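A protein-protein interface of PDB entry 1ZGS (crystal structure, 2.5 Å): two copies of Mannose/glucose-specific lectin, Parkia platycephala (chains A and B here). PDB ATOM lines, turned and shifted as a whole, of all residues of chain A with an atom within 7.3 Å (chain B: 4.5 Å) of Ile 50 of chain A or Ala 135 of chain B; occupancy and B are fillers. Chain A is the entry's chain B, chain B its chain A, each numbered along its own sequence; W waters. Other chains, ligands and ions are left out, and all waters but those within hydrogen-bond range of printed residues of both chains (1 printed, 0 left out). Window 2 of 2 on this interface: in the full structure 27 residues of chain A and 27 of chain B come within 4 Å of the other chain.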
ATOM      1  N   PHE A  21     -15.714 -23.302   8.316  1.00  0.00           N
ATOM      2  CA  PHE A  21     -15.910 -24.455   7.477  1.00  0.00           C
ATOM      3  C   PHE A  21     -15.088 -25.618   8.004  1.00  0.00           C
ATOM      4  O   PHE A  21     -13.862 -25.543   8.054  1.00  0.00           O
ATOM      5  CB  PHE A  21     -15.537 -24.141   6.015  1.00  0.00           C
ATOM      6  CG  PHE A  21     -15.446 -25.367   5.150  1.00  0.00           C
ATOM      7  CD1 PHE A  21     -16.599 -26.065   4.795  1.00  0.00           C
ATOM      8  CD2 PHE A  21     -14.222 -25.854   4.747  1.00  0.00           C
ATOM      9  CE1 PHE A  21     -16.536 -27.225   4.040  1.00  0.00           C
ATOM     10  CE2 PHE A  21     -14.138 -26.995   3.966  1.00  0.00           C
ATOM     11  CZ  PHE A  21     -15.302 -27.691   3.613  1.00  0.00           C
ATOM     12  N   GLU A  29      -8.341 -28.366  -2.118  1.00  0.00           N
ATOM     13  CA  GLU A  29      -8.214 -27.178  -2.949  1.00  0.00           C
ATOM     14  C   GLU A  29      -8.615 -25.935  -2.169  1.00  0.00           C
ATOM     15  O   GLU A  29      -9.559 -25.974  -1.398  1.00  0.00           O
ATOM     16  CB  GLU A  29      -9.043 -27.348  -4.232  1.00  0.00           C
ATOM     17  CG  GLU A  29      -8.906 -26.235  -5.263  1.00  0.00           C
ATOM     18  CD  GLU A  29      -9.876 -26.405  -6.431  1.00  0.00           C
ATOM     19  OE1 GLU A  29      -9.570 -27.149  -7.380  1.00  0.00           O
ATOM     20  OE2 GLU A  29     -10.959 -25.802  -6.409  1.00  0.00           O
ATOM     21  N   VAL A  31      -9.561 -21.946  -3.187  1.00  0.00           N
ATOM     22  CA  VAL A  31      -9.815 -20.993  -4.229  1.00  0.00           C
ATOM     23  C   VAL A  31      -9.895 -19.622  -3.583  1.00  0.00           C
ATOM     24  O   VAL A  31     -10.678 -19.421  -2.641  1.00  0.00           O
ATOM     25  CB  VAL A  31     -11.149 -21.281  -4.976  1.00  0.00           C
ATOM     26  CG1 VAL A  31     -11.355 -20.262  -6.099  1.00  0.00           C
ATOM     27  CG2 VAL A  31     -11.208 -22.748  -5.516  1.00  0.00           C
ATOM     28  N   SER A  42     -12.757 -19.866  -0.802  1.00  0.00           N
ATOM     29  CA  SER A  42     -13.571 -21.066  -0.614  1.00  0.00           C
ATOM     30  C   SER A  42     -12.665 -22.307  -0.654  1.00  0.00           C
ATOM     31  O   SER A  42     -11.455 -22.192  -0.950  1.00  0.00           O
ATOM     32  CB  SER A  42     -14.647 -21.162  -1.691  1.00  0.00           C
ATOM     33  OG  SER A  42     -14.044 -21.382  -2.942  1.00  0.00           O
ATOM     34  N   PHE A  43     -13.243 -23.486  -0.383  1.00  0.00           N
ATOM     35  CA  PHE A  43     -12.441 -24.728  -0.260  1.00  0.00           C
ATOM     36  C   PHE A  43     -13.123 -25.903  -0.897  1.00  0.00           C
ATOM     37  O   PHE A  43     -14.353 -25.905  -1.064  1.00  0.00           O
ATOM     38  CB  PHE A  43     -12.137 -25.061   1.216  1.00  0.00           C
ATOM     39  CG  PHE A  43     -11.745 -23.869   2.011  1.00  0.00           C
ATOM     40  CD1 PHE A  43     -12.717 -23.079   2.622  1.00  0.00           C
ATOM     41  CD2 PHE A  43     -10.403 -23.490   2.106  1.00  0.00           C
ATOM     42  CE1 PHE A  43     -12.360 -21.912   3.326  1.00  0.00           C
ATOM     43  CE2 PHE A  43     -10.020 -22.331   2.819  1.00  0.00           C
ATOM     44  CZ  PHE A  43     -10.997 -21.536   3.422  1.00  0.00           C
ATOM     45  N   LYS A  44     -12.328 -26.918  -1.236  1.00  0.00           N
ATOM     46  CA  LYS A  44     -12.885 -28.175  -1.736  1.00  0.00           C
ATOM     47  C   LYS A  44     -12.183 -29.352  -1.077  1.00  0.00           C
ATOM     48  O   LYS A  44     -10.970 -29.311  -0.890  1.00  0.00           O
ATOM     49  CB  LYS A  44     -12.732 -28.225  -3.245  1.00  0.00           C
ATOM     50  CG  LYS A  44     -13.519 -29.295  -3.995  1.00  0.00           C
ATOM     51  CD  LYS A  44     -13.605 -28.819  -5.425  1.00  0.00           C
ATOM     52  CE  LYS A  44     -13.401 -29.899  -6.450  1.00  0.00           C
ATOM     53  NZ  LYS A  44     -13.509 -29.279  -7.814  1.00  0.00           N
ATOM     54  N   ASP A  45     -12.942 -30.399  -0.738  1.00  0.00           N
ATOM     55  CA  ASP A  45     -12.354 -31.583  -0.125  1.00  0.00           C
ATOM     56  C   ASP A  45     -12.147 -32.757  -1.064  1.00  0.00           C
ATOM     57  O   ASP A  45     -12.562 -32.711  -2.210  1.00  0.00           O
ATOM     58  CB  ASP A  45     -13.109 -31.999   1.140  1.00  0.00           C
ATOM     59  CG  ASP A  45     -14.411 -32.704   0.857  1.00  0.00           C
ATOM     60  OD1 ASP A  45     -14.645 -33.222  -0.289  1.00  0.00           O
ATOM     61  OD2 ASP A  45     -15.269 -32.760   1.768  1.00  0.00           O
ATOM     62  N   SER A  47     -13.485 -35.496  -1.670  1.00  0.00           N
ATOM     63  CA  SER A  47     -14.559 -36.123  -2.398  1.00  0.00           C
ATOM     64  C   SER A  47     -15.411 -35.124  -3.195  1.00  0.00           C
ATOM     65  O   SER A  47     -16.543 -35.451  -3.574  1.00  0.00           O
ATOM     66  CB  SER A  47     -15.394 -37.007  -1.464  1.00  0.00           C
ATOM     67  OG  SER A  47     -15.931 -36.203  -0.449  1.00  0.00           O
ATOM     68  N   GLY A  48     -14.883 -33.924  -3.460  1.00  0.00           N
ATOM     69  CA  GLY A  48     -15.627 -32.920  -4.242  1.00  0.00           C
ATOM     70  C   GLY A  48     -16.565 -31.974  -3.491  1.00  0.00           C
ATOM     71  O   GLY A  48     -17.205 -31.099  -4.105  1.00  0.00           O
ATOM     72  N   ASP A  49     -16.673 -32.125  -2.171  1.00  0.00           N
ATOM     73  CA  ASP A  49     -17.514 -31.222  -1.403  1.00  0.00           C
ATOM     74  C   ASP A  49     -16.881 -29.847  -1.414  1.00  0.00           C
ATOM     75  O   ASP A  49     -15.668 -29.717  -1.299  1.00  0.00           O
ATOM     76  CB  ASP A  49     -17.642 -31.676   0.043  1.00  0.00           C
ATOM     77  CG  ASP A  49     -18.463 -32.951   0.199  1.00  0.00           C
ATOM     78  OD1 ASP A  49     -18.745 -33.632  -0.802  1.00  0.00           O
ATOM     79  OD2 ASP A  49     -18.858 -33.344   1.309  1.00  0.00           O
ATOM     80  N   ILE A  50     -17.707 -28.822  -1.534  1.00  0.00           N
ATOM     81  CA  ILE A  50     -17.208 -27.481  -1.462  1.00  0.00           C
ATOM     82  C   ILE A  50     -17.768 -26.751  -0.253  1.00  0.00           C
ATOM     83  O   ILE A  50     -18.850 -27.083   0.248  1.00  0.00           O
ATOM     84  CB  ILE A  50     -17.536 -26.701  -2.750  1.00  0.00           C
ATOM     85  CG1 ILE A  50     -19.043 -26.728  -3.062  1.00  0.00           C
ATOM     86  CG2 ILE A  50     -16.651 -27.161  -3.933  1.00  0.00           C
ATOM     87  CD1 ILE A  50     -19.484 -25.593  -4.033  1.00  0.00           C
ATOM     88  N   SER A  51     -17.027 -25.756   0.220  1.00  0.00           N
ATOM     89  CA  SER A  51     -17.521 -24.839   1.228  1.00  0.00           C
ATOM     90  C   SER A  51     -18.248 -23.750   0.446  1.00  0.00           C
ATOM     91  O   SER A  51     -18.053 -23.606  -0.768  1.00  0.00           O
ATOM     92  CB  SER A  51     -16.325 -24.237   1.945  1.00  0.00           C
ATOM     93  OG  SER A  51     -15.669 -23.288   1.116  1.00  0.00           O
ATOM     94  N   GLY A  52     -19.042 -22.922   1.061  1.00  0.00           N
ATOM     95  CA  GLY A  52     -19.420 -21.730   0.248  1.00  0.00           C
ATOM     96  C   GLY A  52     -18.219 -20.820  -0.059  1.00  0.00           C
ATOM     97  O   GLY A  52     -17.087 -21.097   0.404  1.00  0.00           O
ATOM     98  N   THR A  53     -18.459 -19.743  -0.829  1.00  0.00           N
ATOM     99  CA  THR A  53     -17.465 -18.673  -1.020  1.00  0.00           C
ATOM    100  C   THR A  53     -17.569 -17.646   0.129  1.00  0.00           C
ATOM    101  O   THR A  53     -18.654 -17.128   0.404  1.00  0.00           O
ATOM    102  CB  THR A  53     -17.665 -18.027  -2.413  1.00  0.00           C
ATOM    103  OG1 THR A  53     -17.257 -18.975  -3.412  1.00  0.00           O
ATOM    104  CG2 THR A  53     -16.740 -16.803  -2.670  1.00  0.00           C
ATOM    105  N   GLY B  16     -22.789 -29.585 -10.587  1.00  0.00           N
ATOM    106  CA  GLY B  16     -22.217 -28.816  -9.478  1.00  0.00           C
ATOM    107  C   GLY B  16     -21.526 -29.692  -8.439  1.00  0.00           C
ATOM    108  O   GLY B  16     -21.360 -30.918  -8.622  1.00  0.00           O
ATOM    109  N   ASN B  17     -21.112 -29.048  -7.356  1.00  0.00           N
ATOM    110  CA  ASN B  17     -20.452 -29.702  -6.248  1.00  0.00           C
ATOM    111  C   ASN B  17     -21.370 -29.720  -5.024  1.00  0.00           C
ATOM    112  O   ASN B  17     -22.088 -28.736  -4.760  1.00  0.00           O
ATOM    113  CB  ASN B  17     -19.165 -28.943  -5.899  1.00  0.00           C
ATOM    114  CG  ASN B  17     -18.148 -28.936  -7.039  1.00  0.00           C
ATOM    115  OD1 ASN B  17     -17.458 -29.918  -7.246  1.00  0.00           O
ATOM    116  ND2 ASN B  17     -18.025 -27.805  -7.747  1.00  0.00           N
ATOM    117  N   TYR B  18     -21.343 -30.827  -4.282  1.00  0.00           N
ATOM    118  CA  TYR B  18     -22.102 -30.952  -3.038  1.00  0.00           C
ATOM    119  C   TYR B  18     -21.665 -29.902  -2.026  1.00  0.00           C
ATOM    120  O   TYR B  18     -20.484 -29.591  -1.895  1.00  0.00           O
ATOM    121  CB  TYR B  18     -21.968 -32.373  -2.427  1.00  0.00           C
ATOM    122  CG  TYR B  18     -22.725 -32.545  -1.123  1.00  0.00           C
ATOM    123  CD1 TYR B  18     -24.078 -32.871  -1.105  1.00  0.00           C
ATOM    124  CD2 TYR B  18     -22.076 -32.347   0.112  1.00  0.00           C
ATOM    125  CE1 TYR B  18     -24.768 -32.989   0.122  1.00  0.00           C
ATOM    126  CE2 TYR B  18     -22.748 -32.470   1.315  1.00  0.00           C
ATOM    127  CZ  TYR B  18     -24.078 -32.799   1.327  1.00  0.00           C
ATOM    128  OH  TYR B  18     -24.714 -32.909   2.558  1.00  0.00           O
ATOM    129  N   TRP B  19     -22.631 -29.344  -1.317  1.00  0.00           N
ATOM    130  CA  TRP B  19     -22.342 -28.457  -0.218  1.00  0.00           C
ATOM    131  C   TRP B  19     -23.425 -28.668   0.852  1.00  0.00           C
ATOM    132  O   TRP B  19     -24.529 -29.160   0.538  1.00  0.00           O
ATOM    133  CB  TRP B  19     -22.298 -27.006  -0.713  1.00  0.00           C
ATOM    134  CG  TRP B  19     -23.601 -26.535  -1.285  1.00  0.00           C
ATOM    135  CD1 TRP B  19     -24.001 -26.588  -2.616  1.00  0.00           C
ATOM    136  CD2 TRP B  19     -24.697 -25.948  -0.569  1.00  0.00           C
ATOM    137  NE1 TRP B  19     -25.267 -26.056  -2.753  1.00  0.00           N
ATOM    138  CE2 TRP B  19     -25.721 -25.657  -1.521  1.00  0.00           C
ATOM    139  CE3 TRP B  19     -24.918 -25.623   0.775  1.00  0.00           C
ATOM    140  CZ2 TRP B  19     -26.945 -25.067  -1.160  1.00  0.00           C
ATOM    141  CZ3 TRP B  19     -26.134 -25.043   1.140  1.00  0.00           C
ATOM    142  CH2 TRP B  19     -27.131 -24.754   0.163  1.00  0.00           C
ATOM    143  N   PHE B  54     -23.331 -20.018  -1.887  1.00  0.00           N
ATOM    144  CA  PHE B  54     -23.301 -21.211  -2.739  1.00  0.00           C
ATOM    145  C   PHE B  54     -23.810 -20.857  -4.135  1.00  0.00           C
ATOM    146  O   PHE B  54     -24.921 -20.334  -4.293  1.00  0.00           O
ATOM    147  CB  PHE B  54     -24.067 -22.405  -2.097  1.00  0.00           C
ATOM    148  CG  PHE B  54     -23.644 -22.685  -0.659  1.00  0.00           C
ATOM    149  CD1 PHE B  54     -24.389 -22.205   0.402  1.00  0.00           C
ATOM    150  CD2 PHE B  54     -22.456 -23.338  -0.381  1.00  0.00           C
ATOM    151  CE1 PHE B  54     -23.997 -22.412   1.706  1.00  0.00           C
ATOM    152  CE2 PHE B  54     -22.056 -23.548   0.929  1.00  0.00           C
ATOM    153  CZ  PHE B  54     -22.823 -23.079   1.968  1.00  0.00           C
ATOM    154  N   GLY B  55     -22.980 -21.133  -5.129  1.00  0.00           N
ATOM    155  CA  GLY B  55     -23.272 -20.801  -6.501  1.00  0.00           C
ATOM    156  C   GLY B  55     -22.738 -19.416  -6.830  1.00  0.00           C
ATOM    157  O   GLY B  55     -21.825 -18.910  -6.149  1.00  0.00           O
ATOM    158  N   LYS B  57     -21.070 -18.397  -9.600  1.00  0.00           N
ATOM    159  CA  LYS B  57     -19.705 -18.374 -10.098  1.00  0.00           C
ATOM    160  C   LYS B  57     -19.624 -18.057 -11.580  1.00  0.00           C
ATOM    161  O   LYS B  57     -18.559 -18.191 -12.177  1.00  0.00           O
ATOM    162  CB  LYS B  57     -18.941 -19.664  -9.758  1.00  0.00           C
ATOM    163  CG  LYS B  57     -18.278 -19.612  -8.381  1.00  0.00           C
ATOM    164  CD  LYS B  57     -17.748 -20.990  -7.950  1.00  0.00           C
ATOM    165  CE  LYS B  57     -17.667 -21.112  -6.406  1.00  0.00           C
ATOM    166  NZ  LYS B  57     -17.195 -22.474  -5.916  1.00  0.00           N
ATOM    167  N   GLY B 133     -27.114 -28.830  -0.881  1.00  0.00           N
ATOM    168  CA  GLY B 133     -27.484 -28.846  -2.278  1.00  0.00           C
ATOM    169  C   GLY B 133     -26.261 -29.033  -3.131  1.00  0.00           C
ATOM    170  O   GLY B 133     -25.227 -29.524  -2.652  1.00  0.00           O
ATOM    171  N   ARG B 134     -26.379 -28.651  -4.403  1.00  0.00           N
ATOM    172  CA  ARG B 134     -25.268 -28.739  -5.340  1.00  0.00           C
ATOM    173  C   ARG B 134     -25.155 -27.379  -5.915  1.00  0.00           C
ATOM    174  O   ARG B 134     -26.180 -26.720  -6.160  1.00  0.00           O
ATOM    175  CB  ARG B 134     -25.557 -29.712  -6.468  1.00  0.00           C
ATOM    176  CG  ARG B 134     -25.839 -31.123  -6.024  1.00  0.00           C
ATOM    177  CD  ARG B 134     -25.579 -32.175  -7.068  1.00  0.00           C
ATOM    178  NE  ARG B 134     -24.799 -33.187  -6.389  1.00  0.00           N
ATOM    179  CZ  ARG B 134     -23.488 -33.382  -6.513  1.00  0.00           C
ATOM    180  NH1 ARG B 134     -22.754 -32.675  -7.369  1.00  0.00           N
ATOM    181  NH2 ARG B 134     -22.908 -34.329  -5.782  1.00  0.00           N
ATOM    182  N   ALA B 135     -23.927 -26.939  -6.148  1.00  0.00           N
ATOM    183  CA  ALA B 135     -23.742 -25.633  -6.752  1.00  0.00           C
ATOM    184  C   ALA B 135     -22.534 -25.588  -7.631  1.00  0.00           C
ATOM    185  O   ALA B 135     -21.551 -26.276  -7.380  1.00  0.00           O
ATOM    186  CB  ALA B 135     -23.702 -24.506  -5.665  1.00  0.00           C
ATOM    187  N   GLY B 136     -22.617 -24.779  -8.679  1.00  0.00           N
ATOM    188  CA  GLY B 136     -21.467 -24.457  -9.546  1.00  0.00           C
ATOM    189  C   GLY B 136     -21.564 -22.981  -9.889  1.00  0.00           C
ATOM    190  O   GLY B 136     -21.405 -22.140  -9.012  1.00  0.00           O
ATOM    191  N   TYR B 138     -24.423 -21.817 -10.831  1.00  0.00           N
ATOM    192  CA  TYR B 138     -25.735 -21.533 -10.310  1.00  0.00           C
ATOM    193  C   TYR B 138     -26.055 -22.492  -9.167  1.00  0.00           C
ATOM    194  O   TYR B 138     -25.225 -23.335  -8.799  1.00  0.00           O
ATOM    195  CB  TYR B 138     -26.779 -21.699 -11.417  1.00  0.00           C
ATOM    196  CG  TYR B 138     -26.387 -21.088 -12.733  1.00  0.00           C
ATOM    197  CD1 TYR B 138     -26.344 -21.869 -13.887  1.00  0.00           C
ATOM    198  CD2 TYR B 138     -26.053 -19.722 -12.826  1.00  0.00           C
ATOM    199  CE1 TYR B 138     -25.985 -21.304 -15.114  1.00  0.00           C
ATOM    200  CE2 TYR B 138     -25.678 -19.151 -14.029  1.00  0.00           C
ATOM    201  CZ  TYR B 138     -25.647 -19.943 -15.175  1.00  0.00           C
ATOM    202  OH  TYR B 138     -25.270 -19.390 -16.388  1.00  0.00           O
ATOM    203  N   ASP B 140     -27.592 -25.616  -8.588  1.00  0.00           N
ATOM    204  CA  ASP B 140     -28.156 -26.767  -9.329  1.00  0.00           C
ATOM    205  C   ASP B 140     -29.244 -27.447  -8.556  1.00  0.00           C
ATOM    206  O   ASP B 140     -30.195 -27.905  -9.172  1.00  0.00           O
ATOM    207  CB  ASP B 140     -27.131 -27.820  -9.716  1.00  0.00           C
ATOM    208  CG  ASP B 140     -25.991 -27.259 -10.538  1.00  0.00           C
ATOM    209  OD1 ASP B 140     -25.252 -26.373 -10.019  1.00  0.00           O
ATOM    210  OD2 ASP B 140     -25.752 -27.678 -11.703  1.00  0.00           O
HETATM  211  O   HOH W   1     -19.760 -32.994  -5.259  1.00  0.00           O
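No position is printed for both chains.
Printed residues of chain A that touch a printed residue of chain B: Gly 48, Asp 49, Ile 50, Ser 51, Gly 52 and Thr 53.
Of the 13 printed residues of chain B, 6 touch a printed residue of chain A.
Printed residues of chain B that touch a printed residue of chain A: Asn 17, Tyr 18, Trp 19, Phe 54, Lys 57 and Ala 135.
Hydrophobic or aromatic side chains of chain B within 4 Å of the printed part of chain A: Tyr 18, Trp 19 and Phe 54.
Among the printed residues, no Asp or Glu carboxylate lies within 4 Å of a Lys or Arg side-chain nitrogen of the other chain.
Water W1 lies within hydrogen-bond range of the backbone NH of Tyr 18 of chain B (2.9 Å), the backbone carbonyl oxygen of Gly 48 of chain A (3.4 Å) and the guanidinium group of Arg 134 of chain B (3.5 Å).
CA of Asp 49 of chain A touches O of Tyr 18 of chain B (3.4 Å).
CB of Asn 17 of chain B touches CG1 of Ile 50 of chain A, at 3.6 Å.
CB of Trp 19 of chain B touches O of Ile 50 of chain A, at 3.6 Å.
Ile 50 of chain A touches Ala 135 of chain B (CD1 to O, 3.99 Å).
CE2 of Phe 54 of chain B touches C of Ser 51 of chain A, at 3.8 Å.
Phe 54 of chain B touches Gly 52 of chain A (CE2 to N, 3.1 Å).
Thr 53 of chain A touches Lys 57 of chain B (OG1 to CE, 3.7 Å).
N of Phe 43 of chain A is in hydrogen-bond range of OG of Ser 51 of chain A (2.9 Å).
The side-chain carboxylate of Asp 45 of chain A is in hydrogen-bond range of the backbone NH of Asp 49 of chain A (3.0 Å).
The backbone NH (N) of Trp 19 of chain B is in hydrogen-bond range of the backbone carbonyl oxygen (O) of Gly 133 of chain B.
The backbone carbonyl oxygen (O) of Ala 135 of chain B is in hydrogen-bond range of the backbone NH (N) of Asn 17 of chain B (2.8 Å).
OD1 of Asp 45 of chain A lies within hydrogen-bond range of N of Gly 48 of chain A (3.3 Å).
Printed residues of chain B within 4 Å of Ile 50 of chain A: Asn 17 (3.6 Å), Tyr 18 (2.9 Å), Trp 19 (3.6 Å) and Ala 135 (3.99 Å).
Of the printed residues of chain A, Ala 135 of chain B touches Ile 50.
Printed residues of chain B within 4 Å of Gly 52 of chain A: Phe 54 (3.1 Å).
Printed residues of chain A within 4 Å of Tyr 18 of chain B: Asp 49 and Ile 50.
Of the printed residues of chain B, Gly 48 of chain A touches Asn 17 (3.4 Å).
Printed residues of chain A within 4 Å of Lys 57 of chain B: Thr 53.
Printed residues of chain B within 4 Å of Thr 53 of chain A: Lys 57.
The nearest printed residue of chain A that does not touch Trp 19 of chain B is Ser 51 of chain A (5.3 Å).
The backbone carbonyl oxygen of Gly 48 of chain A lies close to the side-chain amide oxygen of Asn 17 of chain B.
The backbone NH (N) of Ile 50 of chain A is in hydrogen-bond range of the backbone carbonyl oxygen (O) of Tyr 18 of chain B (2.9 Å).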
